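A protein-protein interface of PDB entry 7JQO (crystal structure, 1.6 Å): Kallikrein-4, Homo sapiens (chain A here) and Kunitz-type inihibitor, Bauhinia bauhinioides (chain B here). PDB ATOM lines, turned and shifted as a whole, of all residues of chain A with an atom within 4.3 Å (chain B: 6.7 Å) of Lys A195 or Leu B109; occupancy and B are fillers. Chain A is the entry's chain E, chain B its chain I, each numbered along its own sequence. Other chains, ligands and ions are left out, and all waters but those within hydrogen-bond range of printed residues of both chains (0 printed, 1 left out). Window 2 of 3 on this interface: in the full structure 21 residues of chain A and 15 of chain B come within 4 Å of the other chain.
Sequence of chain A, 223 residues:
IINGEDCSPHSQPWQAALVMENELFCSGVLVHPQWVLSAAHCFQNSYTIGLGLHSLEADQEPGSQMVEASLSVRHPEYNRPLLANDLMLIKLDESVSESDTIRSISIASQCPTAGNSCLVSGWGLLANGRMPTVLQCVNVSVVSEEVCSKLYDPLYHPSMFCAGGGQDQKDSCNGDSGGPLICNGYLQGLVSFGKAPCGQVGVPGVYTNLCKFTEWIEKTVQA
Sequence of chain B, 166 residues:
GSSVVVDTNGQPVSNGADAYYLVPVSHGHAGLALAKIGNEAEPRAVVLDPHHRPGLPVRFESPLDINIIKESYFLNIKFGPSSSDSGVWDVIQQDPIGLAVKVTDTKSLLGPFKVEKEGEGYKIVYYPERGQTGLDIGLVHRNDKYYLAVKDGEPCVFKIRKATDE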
ATOM      1  N   LEU A 151      14.841  -9.404  -3.025  1.00  0.00           N
ATOM      2  CA  LEU A 151      13.465  -9.292  -2.537  1.00  0.00           C
ATOM      3  C   LEU A 151      12.991  -7.835  -2.525  1.00  0.00           C
ATOM      4  O   LEU A 151      11.798  -7.570  -2.777  1.00  0.00           O
ATOM      5  CB  LEU A 151      13.353  -9.929  -1.139  1.00  0.00           C
ATOM      6  CG  LEU A 151      13.670 -11.440  -1.101  1.00  0.00           C
ATOM      7  CD1 LEU A 151      13.813 -11.990   0.321  1.00  0.00           C
ATOM      8  CD2 LEU A 151      12.681 -12.281  -1.904  1.00  0.00           C
ATOM      9  N   TYR A 152      13.890  -6.885  -2.206  1.00  0.00           N
ATOM     10  CA  TYR A 152      13.437  -5.524  -1.900  1.00  0.00           C
ATOM     11  C   TYR A 152      13.804  -4.462  -2.932  1.00  0.00           C
ATOM     12  O   TYR A 152      13.216  -3.380  -2.876  1.00  0.00           O
ATOM     13  CB  TYR A 152      13.866  -5.074  -0.491  1.00  0.00           C
ATOM     14  CG  TYR A 152      13.033  -5.704   0.605  1.00  0.00           C
ATOM     15  CD1 TYR A 152      11.744  -5.235   0.883  1.00  0.00           C
ATOM     16  CD2 TYR A 152      13.511  -6.790   1.346  1.00  0.00           C
ATOM     17  CE1 TYR A 152      10.980  -5.792   1.900  1.00  0.00           C
ATOM     18  CE2 TYR A 152      12.743  -7.369   2.346  1.00  0.00           C
ATOM     19  CZ  TYR A 152      11.464  -6.876   2.623  1.00  0.00           C
ATOM     20  OH  TYR A 152      10.694  -7.432   3.619  1.00  0.00           O
ATOM     21  N   LEU A 155      13.897  -0.753  -3.570  1.00  0.00           N
ATOM     22  CA  LEU A 155      13.890  -0.028  -2.289  1.00  0.00           C
ATOM     23  C   LEU A 155      14.983  -0.501  -1.340  1.00  0.00           C
ATOM     24  O   LEU A 155      15.108   0.042  -0.258  1.00  0.00           O
ATOM     25  CB  LEU A 155      12.502  -0.087  -1.643  1.00  0.00           C
ATOM     26  CG  LEU A 155      11.422   0.693  -2.396  1.00  0.00           C
ATOM     27  CD1 LEU A 155      10.059   0.492  -1.739  1.00  0.00           C
ATOM     28  CD2 LEU A 155      11.760   2.176  -2.416  1.00  0.00           C
ATOM     29  N   PHE A 193      11.054  -2.048   8.678  1.00  0.00           N
ATOM     30  CA  PHE A 193       9.852  -2.286   7.866  1.00  0.00           C
ATOM     31  C   PHE A 193       9.868  -3.719   7.334  1.00  0.00           C
ATOM     32  O   PHE A 193      10.873  -4.437   7.482  1.00  0.00           O
ATOM     33  CB  PHE A 193       9.708  -1.255   6.715  1.00  0.00           C
ATOM     34  CG  PHE A 193      10.742  -1.377   5.606  1.00  0.00           C
ATOM     35  CD1 PHE A 193      11.945  -0.673   5.681  1.00  0.00           C
ATOM     36  CD2 PHE A 193      10.476  -2.122   4.443  1.00  0.00           C
ATOM     37  CE1 PHE A 193      12.885  -0.753   4.660  1.00  0.00           C
ATOM     38  CE2 PHE A 193      11.425  -2.210   3.412  1.00  0.00           C
ATOM     39  CZ  PHE A 193      12.631  -1.544   3.537  1.00  0.00           C
ATOM     40  N   GLY A 194       8.775  -4.124   6.683  1.00  0.00           N
ATOM     41  CA  GLY A 194       8.794  -5.400   5.993  1.00  0.00           C
ATOM     42  C   GLY A 194       7.577  -5.541   5.098  1.00  0.00           C
ATOM     43  O   GLY A 194       6.664  -4.723   5.158  1.00  0.00           O
ATOM     44  N   LYS A 195       7.556  -6.601   4.295  1.00  0.00           N
ATOM     45  CA  LYS A 195       6.394  -6.942   3.482  1.00  0.00           C
ATOM     46  C   LYS A 195       5.359  -7.598   4.378  1.00  0.00           C
ATOM     47  O   LYS A 195       5.694  -8.512   5.127  1.00  0.00           O
ATOM     48  CB  LYS A 195       6.839  -7.957   2.432  1.00  0.00           C
ATOM     49  CG  LYS A 195       7.885  -7.441   1.470  1.00  0.00           C
ATOM     50  CD  LYS A 195       8.161  -8.391   0.296  1.00  0.00           C
ATOM     51  CE  LYS A 195       9.244  -7.878  -0.631  1.00  0.00           C
ATOM     52  NZ  LYS A 195       9.444  -8.785  -1.790  1.00  0.00           N
ATOM     53  N   ALA A 196       4.104  -7.162   4.281  1.00  0.00           N
ATOM     54  CA  ALA A 196       3.064  -7.692   5.152  1.00  0.00           C
ATOM     55  C   ALA A 196       2.453  -8.914   4.480  1.00  0.00           C
ATOM     56  O   ALA A 196       2.396  -8.962   3.259  1.00  0.00           O
ATOM     57  CB  ALA A 196       2.009  -6.633   5.402  1.00  0.00           C
ATOM     58  N   PRO A 197       1.981  -9.944   5.222  1.00  0.00           N
ATOM     59  CA  PRO A 197       2.028  -9.971   6.690  1.00  0.00           C
ATOM     60  C   PRO A 197       3.379 -10.427   7.245  1.00  0.00           C
ATOM     61  O   PRO A 197       4.194 -11.025   6.543  1.00  0.00           O
ATOM     62  CB  PRO A 197       0.999 -11.063   7.005  1.00  0.00           C
ATOM     63  CG  PRO A 197       1.155 -12.039   5.859  1.00  0.00           C
ATOM     64  CD  PRO A 197       1.362 -11.153   4.650  1.00  0.00           C
ATOM     65  N   GLN A 200       6.230 -14.410   7.243  1.00  0.00           N
ATOM     66  CA  GLN A 200       6.106 -15.208   6.025  1.00  0.00           C
ATOM     67  C   GLN A 200       7.407 -15.964   5.768  1.00  0.00           C
ATOM     68  O   GLN A 200       8.513 -15.388   5.809  1.00  0.00           O
ATOM     69  CB  GLN A 200       5.848 -14.342   4.782  1.00  0.00           C
ATOM     70  CG  GLN A 200       4.494 -13.643   4.761  1.00  0.00           C
ATOM     71  CD  GLN A 200       4.386 -12.824   3.496  1.00  0.00           C
ATOM     72  OE1 GLN A 200       4.165 -13.354   2.411  1.00  0.00           O
ATOM     73  NE2 GLN A 200       4.583 -11.524   3.615  1.00  0.00           N
ATOM     74  N   VAL A 203      10.491 -14.491   3.489  1.00  0.00           N
ATOM     75  CA  VAL A 203      10.412 -13.044   3.383  1.00  0.00           C
ATOM     76  C   VAL A 203      10.967 -12.410   4.660  1.00  0.00           C
ATOM     77  O   VAL A 203      10.286 -12.262   5.657  1.00  0.00           O
ATOM     78  CB  VAL A 203       8.989 -12.532   3.093  1.00  0.00           C
ATOM     79  CG1 VAL A 203       9.038 -11.024   2.782  1.00  0.00           C
ATOM     80  CG2 VAL A 203       8.302 -13.296   1.950  1.00  0.00           C
ATOM     81  N   GLU B  61      -2.470   1.006   4.939  1.00  0.00           N
ATOM     82  CA  GLU B  61      -1.341   0.105   5.167  1.00  0.00           C
ATOM     83  C   GLU B  61      -0.027   0.804   4.789  1.00  0.00           C
ATOM     84  O   GLU B  61       0.120   1.363   3.696  1.00  0.00           O
ATOM     85  CB  GLU B  61      -1.481  -1.178   4.316  1.00  0.00           C
ATOM     86  CG  GLU B  61      -2.718  -2.027   4.683  1.00  0.00           C
ATOM     87  CD  GLU B  61      -2.808  -3.399   4.011  1.00  0.00           C
ATOM     88  OE1 GLU B  61      -2.147  -3.584   2.966  1.00  0.00           O
ATOM     89  OE2 GLU B  61      -3.488  -4.307   4.579  1.00  0.00           O
ATOM     90  N   SER B  62       0.951   0.694   5.686  1.00  0.00           N
ATOM     91  CA  SER B  62       2.338   1.089   5.469  1.00  0.00           C
ATOM     92  C   SER B  62       3.221  -0.127   5.791  1.00  0.00           C
ATOM     93  O   SER B  62       2.932  -0.880   6.735  1.00  0.00           O
ATOM     94  CB  SER B  62       2.685   2.244   6.407  1.00  0.00           C
ATOM     95  OG  SER B  62       4.096   2.417   6.486  1.00  0.00           O
ATOM     96  N   PRO B  63       4.337  -0.346   5.058  1.00  0.00           N
ATOM     97  CA  PRO B  63       5.260  -1.443   5.386  1.00  0.00           C
ATOM     98  C   PRO B  63       6.031  -1.231   6.679  1.00  0.00           C
ATOM     99  O   PRO B  63       6.586  -2.180   7.217  1.00  0.00           O
ATOM    100  CB  PRO B  63       6.210  -1.466   4.168  1.00  0.00           C
ATOM    101  CG  PRO B  63       6.258  -0.047   3.705  1.00  0.00           C
ATOM    102  CD  PRO B  63       4.810   0.464   3.903  1.00  0.00           C
ATOM    103  N   PHE B  74       3.570   7.244   3.028  1.00  0.00           N
ATOM    104  CA  PHE B  74       2.925   6.661   1.856  1.00  0.00           C
ATOM    105  C   PHE B  74       2.144   5.413   2.258  1.00  0.00           C
ATOM    106  O   PHE B  74       2.677   4.529   2.963  1.00  0.00           O
ATOM    107  CB  PHE B  74       3.983   6.270   0.818  1.00  0.00           C
ATOM    108  CG  PHE B  74       4.406   7.435  -0.045  1.00  0.00           C
ATOM    109  CD1 PHE B  74       3.473   8.098  -0.849  1.00  0.00           C
ATOM    110  CD2 PHE B  74       5.731   7.878  -0.043  1.00  0.00           C
ATOM    111  CE1 PHE B  74       3.885   9.162  -1.642  1.00  0.00           C
ATOM    112  CE2 PHE B  74       6.131   8.945  -0.831  1.00  0.00           C
ATOM    113  CZ  PHE B  74       5.204   9.574  -1.636  1.00  0.00           C
ATOM    114  N   ASN B  76      -0.866   2.291   1.137  1.00  0.00           N
ATOM    115  CA  ASN B  76      -1.897   1.627   0.349  1.00  0.00           C
ATOM    116  C   ASN B  76      -3.232   1.827   1.059  1.00  0.00           C
ATOM    117  O   ASN B  76      -3.312   1.876   2.307  1.00  0.00           O
ATOM    118  CB  ASN B  76      -1.626   0.125   0.221  1.00  0.00           C
ATOM    119  CG  ASN B  76      -0.587  -0.143  -0.857  1.00  0.00           C
ATOM    120  OD1 ASN B  76      -0.848   0.192  -2.011  1.00  0.00           O
ATOM    121  ND2 ASN B  76       0.557  -0.748  -0.526  1.00  0.00           N
ATOM    122  N   LYS B 107      -0.542  -5.161  -5.300  1.00  0.00           N
ATOM    123  CA  LYS B 107      -0.185  -4.189  -4.296  1.00  0.00           C
ATOM    124  C   LYS B 107       1.332  -4.000  -4.307  1.00  0.00           C
ATOM    125  O   LYS B 107       2.094  -4.977  -4.252  1.00  0.00           O
ATOM    126  CB  LYS B 107      -0.624  -4.763  -2.949  1.00  0.00           C
ATOM    127  CG  LYS B 107      -0.515  -3.813  -1.774  1.00  0.00           C
ATOM    128  CD  LYS B 107      -1.281  -4.329  -0.584  1.00  0.00           C
ATOM    129  CE  LYS B 107      -0.472  -5.289   0.253  1.00  0.00           C
ATOM    130  NZ  LYS B 107      -1.245  -5.736   1.436  1.00  0.00           N
ATOM    131  N   SER B 108       1.770  -2.744  -4.395  1.00  0.00           N
ATOM    132  CA  SER B 108       3.186  -2.418  -4.229  1.00  0.00           C
ATOM    133  C   SER B 108       3.547  -2.391  -2.748  1.00  0.00           C
ATOM    134  O   SER B 108       2.672  -2.202  -1.900  1.00  0.00           O
ATOM    135  CB  SER B 108       3.582  -1.119  -4.896  1.00  0.00           C
ATOM    136  OG  SER B 108       3.342  -1.182  -6.314  1.00  0.00           O
ATOM    137  N   LEU B 109       4.838  -2.575  -2.428  1.00  0.00           N
ATOM    138  CA  LEU B 109       5.269  -2.457  -1.039  1.00  0.00           C
ATOM    139  C   LEU B 109       4.869  -1.105  -0.438  1.00  0.00           C
ATOM    140  O   LEU B 109       4.429  -1.020   0.718  1.00  0.00           O
ATOM    141  CB  LEU B 109       6.789  -2.666  -0.947  1.00  0.00           C
ATOM    142  CG  LEU B 109       7.392  -2.559   0.452  1.00  0.00           C
ATOM    143  CD1 LEU B 109       6.969  -3.759   1.295  1.00  0.00           C
ATOM    144  CD2 LEU B 109       8.916  -2.524   0.357  1.00  0.00           C
ATOM    145  N   LEU B 110       5.045  -0.038  -1.221  1.00  0.00           N
ATOM    146  CA  LEU B 110       4.710   1.305  -0.806  1.00  0.00           C
ATOM    147  C   LEU B 110       3.602   1.791  -1.726  1.00  0.00           C
ATOM    148  O   LEU B 110       3.768   1.816  -2.953  1.00  0.00           O
ATOM    149  CB  LEU B 110       5.988   2.100  -1.048  1.00  0.00           C
ATOM    150  CG  LEU B 110       6.324   3.238  -0.129  1.00  0.00           C
ATOM    151  CD1 LEU B 110       6.104   2.892   1.332  1.00  0.00           C
ATOM    152  CD2 LEU B 110       7.758   3.657  -0.409  1.00  0.00           C
ATOM    153  N   GLY B 111       2.453   2.136  -1.128  1.00  0.00           N
ATOM    154  CA  GLY B 111       1.364   2.682  -1.923  1.00  0.00           C
ATOM    155  C   GLY B 111       1.596   4.152  -2.277  1.00  0.00           C
ATOM    156  O   GLY B 111       2.546   4.795  -1.817  1.00  0.00           O
ATOM    157  N   ARG B 130       5.158   8.259  -6.524  1.00  0.00           N
ATOM    158  CA  ARG B 130       5.603   8.458  -5.142  1.00  0.00           C
ATOM    159  C   ARG B 130       6.627   9.594  -5.074  1.00  0.00           C
ATOM    160  O   ARG B 130       7.579   9.531  -4.286  1.00  0.00           O
ATOM    161  CB  ARG B 130       6.184   7.175  -4.540  1.00  0.00           C
ATOM    162  CG  ARG B 130       5.147   6.093  -4.286  1.00  0.00           C
ATOM    163  CD  ARG B 130       4.330   5.558  -5.419  1.00  0.00           C
ATOM    164  NE  ARG B 130       3.889   4.204  -5.079  1.00  0.00           N
ATOM    165  CZ  ARG B 130       3.099   3.465  -5.849  1.00  0.00           C
ATOM    166  NH1 ARG B 130       2.786   2.250  -5.455  1.00  0.00           N
ATOM    167  NH2 ARG B 130       2.674   3.914  -7.024  1.00  0.00           N
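The backbone carbonyl oxygen (O) of Leu A151 is in hydrogen-bond range of the side-chain amino group (NZ) of Lys A195 (2.8 Å).
The side-chain hydroxyl (OH) of Tyr A152 lies within hydrogen-bond range of the backbone NH (N) of Lys A195.
Lys A195 touches just one residue of chain B: Leu B109 (3.8 Å).
Of the printed residues of chain A, Leu B109 touches Tyr A152, Leu A155, Phe A193, Gly A194 and Lys A195.
Of the printed residues of chain B, Tyr A152 touches Leu B109 (3.95 Å).
Of the printed residues of chain B, Phe A193 touches Pro B63 (3.3 Å) and Leu B109 (3.97 Å).
Of the printed residues of chain A, Pro B63 touches Phe A193 (3.3 Å) and Gly A194 (3.0 Å).
Gly B111 touches none of the printed residues of chain A.
Printed residues of chain A that touch a printed residue of chain B: Tyr A152, Leu A155, Phe A193, Gly A194 and Lys A195.
Hydrophobic or aromatic side chains of chain A that line the printed part of chain B: Tyr A152, Leu A155 and Phe A193.
Printed residues of chain B that touch a printed residue of chain A: Pro B63 and Leu B109.
Hydrophobic or aromatic side chains of chain B that line the printed part of chain A: Pro B63 and Leu B109.
Leu B109 touches Tyr A152 (CD2 to CD1, 3.95 Å).
Leu B109 touches Leu A155.
Phe A193 touches Pro B63 (CB to O, 3.3 Å).
Phe A193 touches Leu B109 (CE2 to CD2, 3.97 Å).
O of Gly A194 touches CD1 of Leu B109, 3.99 Å away.
Lys A195 touches Leu B109 (CG to CD1, 3.8 Å).
N of Gly A194 is in hydrogen-bond range of O of Pro B63 (3.0 Å).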
